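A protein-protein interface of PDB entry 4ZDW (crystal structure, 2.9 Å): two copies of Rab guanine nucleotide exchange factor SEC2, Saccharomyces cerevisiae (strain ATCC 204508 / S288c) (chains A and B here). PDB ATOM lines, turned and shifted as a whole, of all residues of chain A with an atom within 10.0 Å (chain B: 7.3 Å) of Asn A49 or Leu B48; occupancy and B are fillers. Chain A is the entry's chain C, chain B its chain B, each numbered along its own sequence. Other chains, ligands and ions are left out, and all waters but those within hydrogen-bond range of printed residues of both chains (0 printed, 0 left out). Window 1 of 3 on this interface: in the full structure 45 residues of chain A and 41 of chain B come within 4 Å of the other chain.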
ATOM      1  N   ALA A  41      29.848 -14.899   4.463  1.00  0.00           N
ATOM      2  CA  ALA A  41      28.920 -14.368   3.464  1.00  0.00           C
ATOM      3  C   ALA A  41      28.396 -15.467   2.544  1.00  0.00           C
ATOM      4  O   ALA A  41      27.267 -15.397   2.063  1.00  0.00           O
ATOM      5  CB  ALA A  41      29.550 -13.240   2.667  1.00  0.00           C
ATOM      6  N   GLU A  42      29.218 -16.486   2.310  1.00  0.00           N
ATOM      7  CA  GLU A  42      28.782 -17.682   1.582  1.00  0.00           C
ATOM      8  C   GLU A  42      27.945 -18.553   2.505  1.00  0.00           C
ATOM      9  O   GLU A  42      26.943 -19.129   2.093  1.00  0.00           O
ATOM     10  CB  GLU A  42      29.990 -18.476   1.066  1.00  0.00           C
ATOM     11  CG  GLU A  42      30.996 -17.644   0.269  1.00  0.00           C
ATOM     12  CD  GLU A  42      32.168 -18.455  -0.277  1.00  0.00           C
ATOM     13  OE1 GLU A  42      32.398 -18.407  -1.503  1.00  0.00           O
ATOM     14  OE2 GLU A  42      32.868 -19.135   0.502  1.00  0.00           O
ATOM     15  N   GLU A  43      28.368 -18.618   3.764  1.00  0.00           N
ATOM     16  CA  GLU A  43      27.768 -19.479   4.781  1.00  0.00           C
ATOM     17  C   GLU A  43      26.264 -19.229   4.929  1.00  0.00           C
ATOM     18  O   GLU A  43      25.457 -20.169   5.045  1.00  0.00           O
ATOM     19  CB  GLU A  43      28.495 -19.272   6.129  1.00  0.00           C
ATOM     20  CG  GLU A  43      28.681 -20.513   7.003  1.00  0.00           C
ATOM     21  CD  GLU A  43      29.339 -21.684   6.269  1.00  0.00           C
ATOM     22  OE1 GLU A  43      30.541 -21.947   6.533  1.00  0.00           O
ATOM     23  OE2 GLU A  43      28.660 -22.341   5.431  1.00  0.00           O
ATOM     24  N   GLU A  44      25.892 -17.957   4.915  1.00  0.00           N
ATOM     25  CA  GLU A  44      24.509 -17.604   5.109  1.00  0.00           C
ATOM     26  C   GLU A  44      23.707 -17.671   3.809  1.00  0.00           C
ATOM     27  O   GLU A  44      22.568 -18.108   3.808  1.00  0.00           O
ATOM     28  CB  GLU A  44      24.377 -16.267   5.842  1.00  0.00           C
ATOM     29  CG  GLU A  44      24.699 -15.027   5.026  1.00  0.00           C
ATOM     30  CD  GLU A  44      24.749 -13.783   5.898  1.00  0.00           C
ATOM     31  OE1 GLU A  44      23.811 -12.950   5.820  1.00  0.00           O
ATOM     32  OE2 GLU A  44      25.722 -13.646   6.680  1.00  0.00           O
ATOM     33  N   ALA A  45      24.298 -17.266   2.692  1.00  0.00           N
ATOM     34  CA  ALA A  45      23.568 -17.311   1.428  1.00  0.00           C
ATOM     35  C   ALA A  45      23.148 -18.727   1.119  1.00  0.00           C
ATOM     36  O   ALA A  45      22.108 -18.932   0.524  1.00  0.00           O
ATOM     37  CB  ALA A  45      24.370 -16.712   0.282  1.00  0.00           C
ATOM     38  N   ASP A  46      23.948 -19.699   1.541  1.00  0.00           N
ATOM     39  CA  ASP A  46      23.551 -21.108   1.464  1.00  0.00           C
ATOM     40  C   ASP A  46      22.396 -21.381   2.370  1.00  0.00           C
ATOM     41  O   ASP A  46      21.361 -21.829   1.908  1.00  0.00           O
ATOM     42  CB  ASP A  46      24.683 -22.035   1.868  1.00  0.00           C
ATOM     43  CG  ASP A  46      25.605 -22.325   0.732  1.00  0.00           C
ATOM     44  OD1 ASP A  46      26.194 -21.350   0.192  1.00  0.00           O
ATOM     45  OD2 ASP A  46      25.728 -23.523   0.377  1.00  0.00           O
ATOM     46  N   LYS A  47      22.592 -21.112   3.659  1.00  0.00           N
ATOM     47  CA  LYS A  47      21.551 -21.244   4.669  1.00  0.00           C
ATOM     48  C   LYS A  47      20.221 -20.798   4.103  1.00  0.00           C
ATOM     49  O   LYS A  47      19.215 -21.503   4.244  1.00  0.00           O
ATOM     50  CB  LYS A  47      21.895 -20.409   5.909  1.00  0.00           C
ATOM     51  CG  LYS A  47      20.698 -20.017   6.761  1.00  0.00           C
ATOM     52  CD  LYS A  47      21.075 -19.773   8.210  1.00  0.00           C
ATOM     53  CE  LYS A  47      20.076 -20.473   9.122  1.00  0.00           C
ATOM     54  NZ  LYS A  47      20.360 -20.218  10.559  1.00  0.00           N
ATOM     55  N   LEU A  48      20.242 -19.638   3.448  1.00  0.00           N
ATOM     56  CA  LEU A  48      19.056 -19.018   2.889  1.00  0.00           C
ATOM     57  C   LEU A  48      18.455 -19.858   1.774  1.00  0.00           C
ATOM     58  O   LEU A  48      17.296 -20.229   1.842  1.00  0.00           O
ATOM     59  CB  LEU A  48      19.383 -17.621   2.364  1.00  0.00           C
ATOM     60  CG  LEU A  48      18.215 -16.766   1.859  1.00  0.00           C
ATOM     61  CD1 LEU A  48      17.074 -17.001   2.823  1.00  0.00           C
ATOM     62  CD2 LEU A  48      18.513 -15.263   1.719  1.00  0.00           C
ATOM     63  N   ASN A  49      19.229 -20.162   0.743  1.00  0.00           N
ATOM     64  CA  ASN A  49      18.647 -20.827  -0.409  1.00  0.00           C
ATOM     65  C   ASN A  49      18.262 -22.205  -0.026  1.00  0.00           C
ATOM     66  O   ASN A  49      17.343 -22.749  -0.627  1.00  0.00           O
ATOM     67  CB  ASN A  49      19.561 -20.822  -1.627  1.00  0.00           C
ATOM     68  CG  ASN A  49      20.018 -19.422  -1.994  1.00  0.00           C
ATOM     69  OD1 ASN A  49      19.887 -18.502  -1.207  1.00  0.00           O
ATOM     70  ND2 ASN A  49      20.562 -19.262  -3.183  1.00  0.00           N
ATOM     71  N   LYS A  50      18.924 -22.743   1.000  1.00  0.00           N
ATOM     72  CA  LYS A  50      18.479 -23.996   1.615  1.00  0.00           C
ATOM     73  C   LYS A  50      17.015 -23.858   2.039  1.00  0.00           C
ATOM     74  O   LYS A  50      16.174 -24.665   1.627  1.00  0.00           O
ATOM     75  CB  LYS A  50      19.353 -24.434   2.803  1.00  0.00           C
ATOM     76  CG  LYS A  50      20.784 -24.933   2.508  1.00  0.00           C
ATOM     77  CD  LYS A  50      21.002 -25.552   1.124  1.00  0.00           C
ATOM     78  CE  LYS A  50      20.215 -26.846   0.918  1.00  0.00           C
ATOM     79  NZ  LYS A  50      19.422 -26.831  -0.356  1.00  0.00           N
ATOM     80  N   GLU A  51      16.715 -22.818   2.821  1.00  0.00           N
ATOM     81  CA  GLU A  51      15.338 -22.500   3.237  1.00  0.00           C
ATOM     82  C   GLU A  51      14.401 -22.239   2.064  1.00  0.00           C
ATOM     83  O   GLU A  51      13.269 -22.690   2.069  1.00  0.00           O
ATOM     84  CB  GLU A  51      15.306 -21.310   4.198  1.00  0.00           C
ATOM     85  CG  GLU A  51      15.734 -21.683   5.608  1.00  0.00           C
ATOM     86  CD  GLU A  51      15.772 -20.513   6.593  1.00  0.00           C
ATOM     87  OE1 GLU A  51      16.591 -20.570   7.550  1.00  0.00           O
ATOM     88  OE2 GLU A  51      14.984 -19.547   6.436  1.00  0.00           O
ATOM     89  N   VAL A  52      14.871 -21.527   1.049  1.00  0.00           N
ATOM     90  CA  VAL A  52      14.017 -21.202  -0.083  1.00  0.00           C
ATOM     91  C   VAL A  52      13.764 -22.423  -0.964  1.00  0.00           C
ATOM     92  O   VAL A  52      12.666 -22.602  -1.469  1.00  0.00           O
ATOM     93  CB  VAL A  52      14.539 -19.974  -0.845  1.00  0.00           C
ATOM     94  CG1 VAL A  52      13.812 -19.766  -2.163  1.00  0.00           C
ATOM     95  CG2 VAL A  52      14.339 -18.768   0.037  1.00  0.00           C
ATOM     96  N   GLU A  53      14.767 -23.278  -1.129  1.00  0.00           N
ATOM     97  CA  GLU A  53      14.521 -24.557  -1.785  1.00  0.00           C
ATOM     98  C   GLU A  53      13.564 -25.369  -0.919  1.00  0.00           C
ATOM     99  O   GLU A  53      12.657 -26.016  -1.431  1.00  0.00           O
ATOM    100  CB  GLU A  53      15.818 -25.333  -2.025  1.00  0.00           C
ATOM    101  CG  GLU A  53      16.652 -24.829  -3.208  1.00  0.00           C
ATOM    102  CD  GLU A  53      18.139 -25.223  -3.117  1.00  0.00           C
ATOM    103  OE1 GLU A  53      18.443 -26.445  -3.052  1.00  0.00           O
ATOM    104  OE2 GLU A  53      19.014 -24.306  -3.112  1.00  0.00           O
ATOM    105  N   ASP A  54      13.744 -25.290   0.392  1.00  0.00           N
ATOM    106  CA  ASP A  54      12.905 -26.038   1.292  1.00  0.00           C
ATOM    107  C   ASP A  54      11.447 -25.602   1.228  1.00  0.00           C
ATOM    108  O   ASP A  54      10.545 -26.427   1.187  1.00  0.00           O
ATOM    109  CB  ASP A  54      13.409 -25.961   2.731  1.00  0.00           C
ATOM    110  CG  ASP A  54      12.540 -26.765   3.697  1.00  0.00           C
ATOM    111  OD1 ASP A  54      11.972 -27.807   3.287  1.00  0.00           O
ATOM    112  OD2 ASP A  54      12.418 -26.350   4.867  1.00  0.00           O
ATOM    113  N   LEU A  55      11.205 -24.312   1.238  1.00  0.00           N
ATOM    114  CA  LEU A  55       9.860 -23.809   1.122  1.00  0.00           C
ATOM    115  C   LEU A  55       9.219 -24.277  -0.192  1.00  0.00           C
ATOM    116  O   LEU A  55       8.049 -24.628  -0.241  1.00  0.00           O
ATOM    117  CB  LEU A  55       9.943 -22.283   1.155  1.00  0.00           C
ATOM    118  CG  LEU A  55       8.727 -21.379   1.071  1.00  0.00           C
ATOM    119  CD1 LEU A  55       7.792 -21.749   2.212  1.00  0.00           C
ATOM    120  CD2 LEU A  55       9.125 -19.907   1.131  1.00  0.00           C
ATOM    121  N   THR A  56       9.994 -24.298  -1.264  1.00  0.00           N
ATOM    122  CA  THR A  56       9.397 -24.246  -2.587  1.00  0.00           C
ATOM    123  C   THR A  56       8.905 -25.623  -2.864  1.00  0.00           C
ATOM    124  O   THR A  56       7.828 -25.763  -3.359  1.00  0.00           O
ATOM    125  CB  THR A  56      10.349 -23.647  -3.675  1.00  0.00           C
ATOM    126  OG1 THR A  56      10.811 -22.385  -3.235  1.00  0.00           O
ATOM    127  CG2 THR A  56       9.649 -23.388  -4.966  1.00  0.00           C
ATOM    128  N   ALA A  57       9.670 -26.631  -2.472  1.00  0.00           N
ATOM    129  CA  ALA A  57       9.213 -28.037  -2.553  1.00  0.00           C
ATOM    130  C   ALA A  57       7.952 -28.266  -1.733  1.00  0.00           C
ATOM    131  O   ALA A  57       6.944 -28.807  -2.245  1.00  0.00           O
ATOM    132  CB  ALA A  57      10.285 -28.988  -2.058  1.00  0.00           C
ATOM    133  N   GLU B  43      27.829  -8.742  -1.048  1.00  0.00           N
ATOM    134  CA  GLU B  43      26.861  -8.090  -1.918  1.00  0.00           C
ATOM    135  C   GLU B  43      25.752  -9.071  -2.251  1.00  0.00           C
ATOM    136  O   GLU B  43      24.575  -8.736  -2.152  1.00  0.00           O
ATOM    137  CB  GLU B  43      27.513  -7.607  -3.211  1.00  0.00           C
ATOM    138  CG  GLU B  43      28.136  -6.224  -3.163  1.00  0.00           C
ATOM    139  CD  GLU B  43      29.032  -5.972  -4.376  1.00  0.00           C
ATOM    140  OE1 GLU B  43      28.952  -6.755  -5.357  1.00  0.00           O
ATOM    141  OE2 GLU B  43      29.828  -4.998  -4.356  1.00  0.00           O
ATOM    142  N   GLU B  44      26.145 -10.274  -2.663  1.00  0.00           N
ATOM    143  CA  GLU B  44      25.205 -11.383  -2.829  1.00  0.00           C
ATOM    144  C   GLU B  44      24.372 -11.663  -1.575  1.00  0.00           C
ATOM    145  O   GLU B  44      23.148 -11.667  -1.628  1.00  0.00           O
ATOM    146  CB  GLU B  44      25.932 -12.652  -3.265  1.00  0.00           C
ATOM    147  CG  GLU B  44      25.034 -13.629  -4.013  1.00  0.00           C
ATOM    148  CD  GLU B  44      24.330 -13.001  -5.217  1.00  0.00           C
ATOM    149  OE1 GLU B  44      24.883 -12.037  -5.818  1.00  0.00           O
ATOM    150  OE2 GLU B  44      23.223 -13.470  -5.565  1.00  0.00           O
ATOM    151  N   ALA B  45      25.042 -11.894  -0.457  1.00  0.00           N
ATOM    152  CA  ALA B  45      24.380 -11.982   0.837  1.00  0.00           C
ATOM    153  C   ALA B  45      23.211 -11.026   0.903  1.00  0.00           C
ATOM    154  O   ALA B  45      22.055 -11.414   1.063  1.00  0.00           O
ATOM    155  CB  ALA B  45      25.371 -11.620   1.933  1.00  0.00           C
ATOM    156  N   ASP B  46      23.555  -9.756   0.769  1.00  0.00           N
ATOM    157  CA  ASP B  46      22.634  -8.655   0.875  1.00  0.00           C
ATOM    158  C   ASP B  46      21.545  -8.703  -0.209  1.00  0.00           C
ATOM    159  O   ASP B  46      20.356  -8.576   0.089  1.00  0.00           O
ATOM    160  CB  ASP B  46      23.447  -7.365   0.780  1.00  0.00           C
ATOM    161  CG  ASP B  46      22.650  -6.143   1.148  1.00  0.00           C
ATOM    162  OD1 ASP B  46      21.538  -6.273   1.714  1.00  0.00           O
ATOM    163  OD2 ASP B  46      23.137  -5.032   0.870  1.00  0.00           O
ATOM    164  N   LYS B  47      21.958  -8.900  -1.458  1.00  0.00           N
ATOM    165  CA  LYS B  47      21.060  -8.806  -2.593  1.00  0.00           C
ATOM    166  C   LYS B  47      19.917  -9.767  -2.390  1.00  0.00           C
ATOM    167  O   LYS B  47      18.753  -9.370  -2.432  1.00  0.00           O
ATOM    168  CB  LYS B  47      21.810  -9.093  -3.888  1.00  0.00           C
ATOM    169  CG  LYS B  47      20.960  -9.063  -5.143  1.00  0.00           C
ATOM    170  CD  LYS B  47      21.745  -9.633  -6.319  1.00  0.00           C
ATOM    171  CE  LYS B  47      20.838 -10.304  -7.349  1.00  0.00           C
ATOM    172  NZ  LYS B  47      20.212  -9.318  -8.281  1.00  0.00           N
ATOM    173  N   LEU B  48      20.258 -11.020  -2.118  1.00  0.00           N
ATOM    174  CA  LEU B  48      19.261 -12.044  -1.854  1.00  0.00           C
ATOM    175  C   LEU B  48      18.378 -11.678  -0.687  1.00  0.00           C
ATOM    176  O   LEU B  48      17.146 -11.717  -0.786  1.00  0.00           O
ATOM    177  CB  LEU B  48      19.912 -13.390  -1.565  1.00  0.00           C
ATOM    178  CG  LEU B  48      20.877 -13.984  -2.599  1.00  0.00           C
ATOM    179  CD1 LEU B  48      21.113 -15.464  -2.287  1.00  0.00           C
ATOM    180  CD2 LEU B  48      20.409 -13.757  -4.046  1.00  0.00           C
ATOM    181  N   ASN B  49      19.000 -11.320   0.425  1.00  0.00           N
ATOM    182  CA  ASN B  49      18.231 -10.892   1.573  1.00  0.00           C
ATOM    183  C   ASN B  49      17.129  -9.896   1.246  1.00  0.00           C
ATOM    184  O   ASN B  49      16.047  -9.994   1.815  1.00  0.00           O
ATOM    185  CB  ASN B  49      19.130 -10.366   2.679  1.00  0.00           C
ATOM    186  CG  ASN B  49      19.499 -11.442   3.676  1.00  0.00           C
ATOM    187  OD1 ASN B  49      18.686 -12.330   3.985  1.00  0.00           O
ATOM    188  ND2 ASN B  49      20.731 -11.375   4.193  1.00  0.00           N
ATOM    189  N   LYS B  50      17.396  -8.962   0.327  1.00  0.00           N
ATOM    190  CA  LYS B  50      16.372  -8.011  -0.118  1.00  0.00           C
ATOM    191  C   LYS B  50      15.335  -8.655  -1.057  1.00  0.00           C
ATOM    192  O   LYS B  50      14.133  -8.696  -0.742  1.00  0.00           O
ATOM    193  CB  LYS B  50      17.007  -6.785  -0.748  1.00  0.00           C
ATOM    194  CG  LYS B  50      17.914  -6.051   0.214  1.00  0.00           C
ATOM    195  CD  LYS B  50      18.054  -4.578  -0.146  1.00  0.00           C
ATOM    196  CE  LYS B  50      19.360  -4.019   0.431  1.00  0.00           C
ATOM    197  NZ  LYS B  50      19.391  -2.530   0.428  1.00  0.00           N
ATOM    198  N   GLU B  51      15.808  -9.183  -2.184  1.00  0.00           N
ATOM    199  CA  GLU B  51      14.954  -9.853  -3.194  1.00  0.00           C
ATOM    200  C   GLU B  51      13.926 -10.930  -2.714  1.00  0.00           C
ATOM    201  O   GLU B  51      12.931 -11.190  -3.404  1.00  0.00           O
ATOM    202  CB  GLU B  51      15.848 -10.425  -4.311  1.00  0.00           C
ATOM    203  CG  GLU B  51      16.439  -9.344  -5.199  1.00  0.00           C
ATOM    204  CD  GLU B  51      17.414  -9.865  -6.243  1.00  0.00           C
ATOM    205  OE1 GLU B  51      17.871 -11.026  -6.106  1.00  0.00           O
ATOM    206  OE2 GLU B  51      17.731  -9.091  -7.194  1.00  0.00           O
ATOM    207  N   VAL B  52      14.169 -11.510  -1.538  1.00  0.00           N
ATOM    208  CA  VAL B  52      13.459 -12.698  -1.034  1.00  0.00           C
ATOM    209  C   VAL B  52      11.945 -12.595  -0.694  1.00  0.00           C
ATOM    210  O   VAL B  52      11.169 -13.489  -1.055  1.00  0.00           O
ATOM    211  CB  VAL B  52      14.221 -13.253   0.178  1.00  0.00           C
ATOM    212  CG1 VAL B  52      14.332 -12.181   1.247  1.00  0.00           C
ATOM    213  CG2 VAL B  52      13.577 -14.518   0.726  1.00  0.00           C
ATOM    214  N   GLU B  53      11.527 -11.539   0.011  1.00  0.00           N
ATOM    215  CA  GLU B  53      10.101 -11.347   0.327  1.00  0.00           C
ATOM    216  C   GLU B  53       9.349 -11.504  -0.979  1.00  0.00           C
ATOM    217  O   GLU B  53       8.652 -12.494  -1.165  1.00  0.00           O
ATOM    218  CB  GLU B  53       9.832  -9.969   0.961  1.00  0.00           C
ATOM    219  CG  GLU B  53       8.348  -9.674   1.225  1.00  0.00           C
ATOM    220  CD  GLU B  53       8.077  -8.354   1.961  1.00  0.00           C
ATOM    221  OE1 GLU B  53       9.034  -7.651   2.343  1.00  0.00           O
ATOM    222  OE2 GLU B  53       6.893  -8.012   2.166  1.00  0.00           O
ATOM    223  N   LEU B  55      10.110 -12.577  -3.851  1.00  0.00           N
ATOM    224  CA  LEU B  55      10.242 -13.887  -4.448  1.00  0.00           C
ATOM    225  C   LEU B  55       9.313 -14.860  -3.766  1.00  0.00           C
ATOM    226  O   LEU B  55       8.742 -15.725  -4.405  1.00  0.00           O
ATOM    227  CB  LEU B  55      11.686 -14.377  -4.317  1.00  0.00           C
ATOM    228  CG  LEU B  55      12.090 -15.764  -4.834  1.00  0.00           C
ATOM    229  CD1 LEU B  55      11.879 -16.818  -3.752  1.00  0.00           C
ATOM    230  CD2 LEU B  55      11.336 -16.119  -6.120  1.00  0.00           C
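O of Ala B45 sits at hydrogen-bond distance from ND2 of Asn B49.
The side-chain amide oxygen (OD1) of Asn A49 lies close to the backbone carbonyl oxygen (O) of Ala A45 (2.8 Å).
O of Val A52 lies within hydrogen-bond range of OG1 of Thr A56, at 2.6 Å.
Among the printed residues, pairs that only touch across the chains: Asn A49 with Leu B48, Leu A48 with Asn B49, Glu A44 with Asn B49 and Val A52 with Leu B55.
Of the printed residues of chain B, Glu A44 touches Asn B49 (3.8 Å).
Of the printed residues of chain B, Leu A48 touches Asn B49.
Printed residues of chain B within 4 Å of Val A52: Leu B55.
Leu B48 touches just one residue of chain A: Asn A49.
Of the printed residues of chain A, Asn B49 touches Glu A44 and Leu A48.
Of the printed residues of chain A, Leu B55 touches Val A52.
The nearest residue of chain B that does not touch Asn A49 is Glu B44 (6.8 Å).
The nearest residue of chain A that does not touch Leu B48 is Leu A48 (4.03 Å).
Among the printed residues, no Asp or Glu carboxylate lies within 4 Å of a Lys or Arg side-chain nitrogen of the other chain.
Glu A44 touches Asn B49, but with the chains exchanged Asn A49 does not touch Glu B44 (6.8 Å).
Leu A48 touches Asn B49, and with the chains exchanged Asn A49 touches Leu B48.
Val A52 touches Leu B55, but with the chains exchanged Leu A55 does not touch Val B52 (7.0 Å).
12 positions are printed for both chains.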
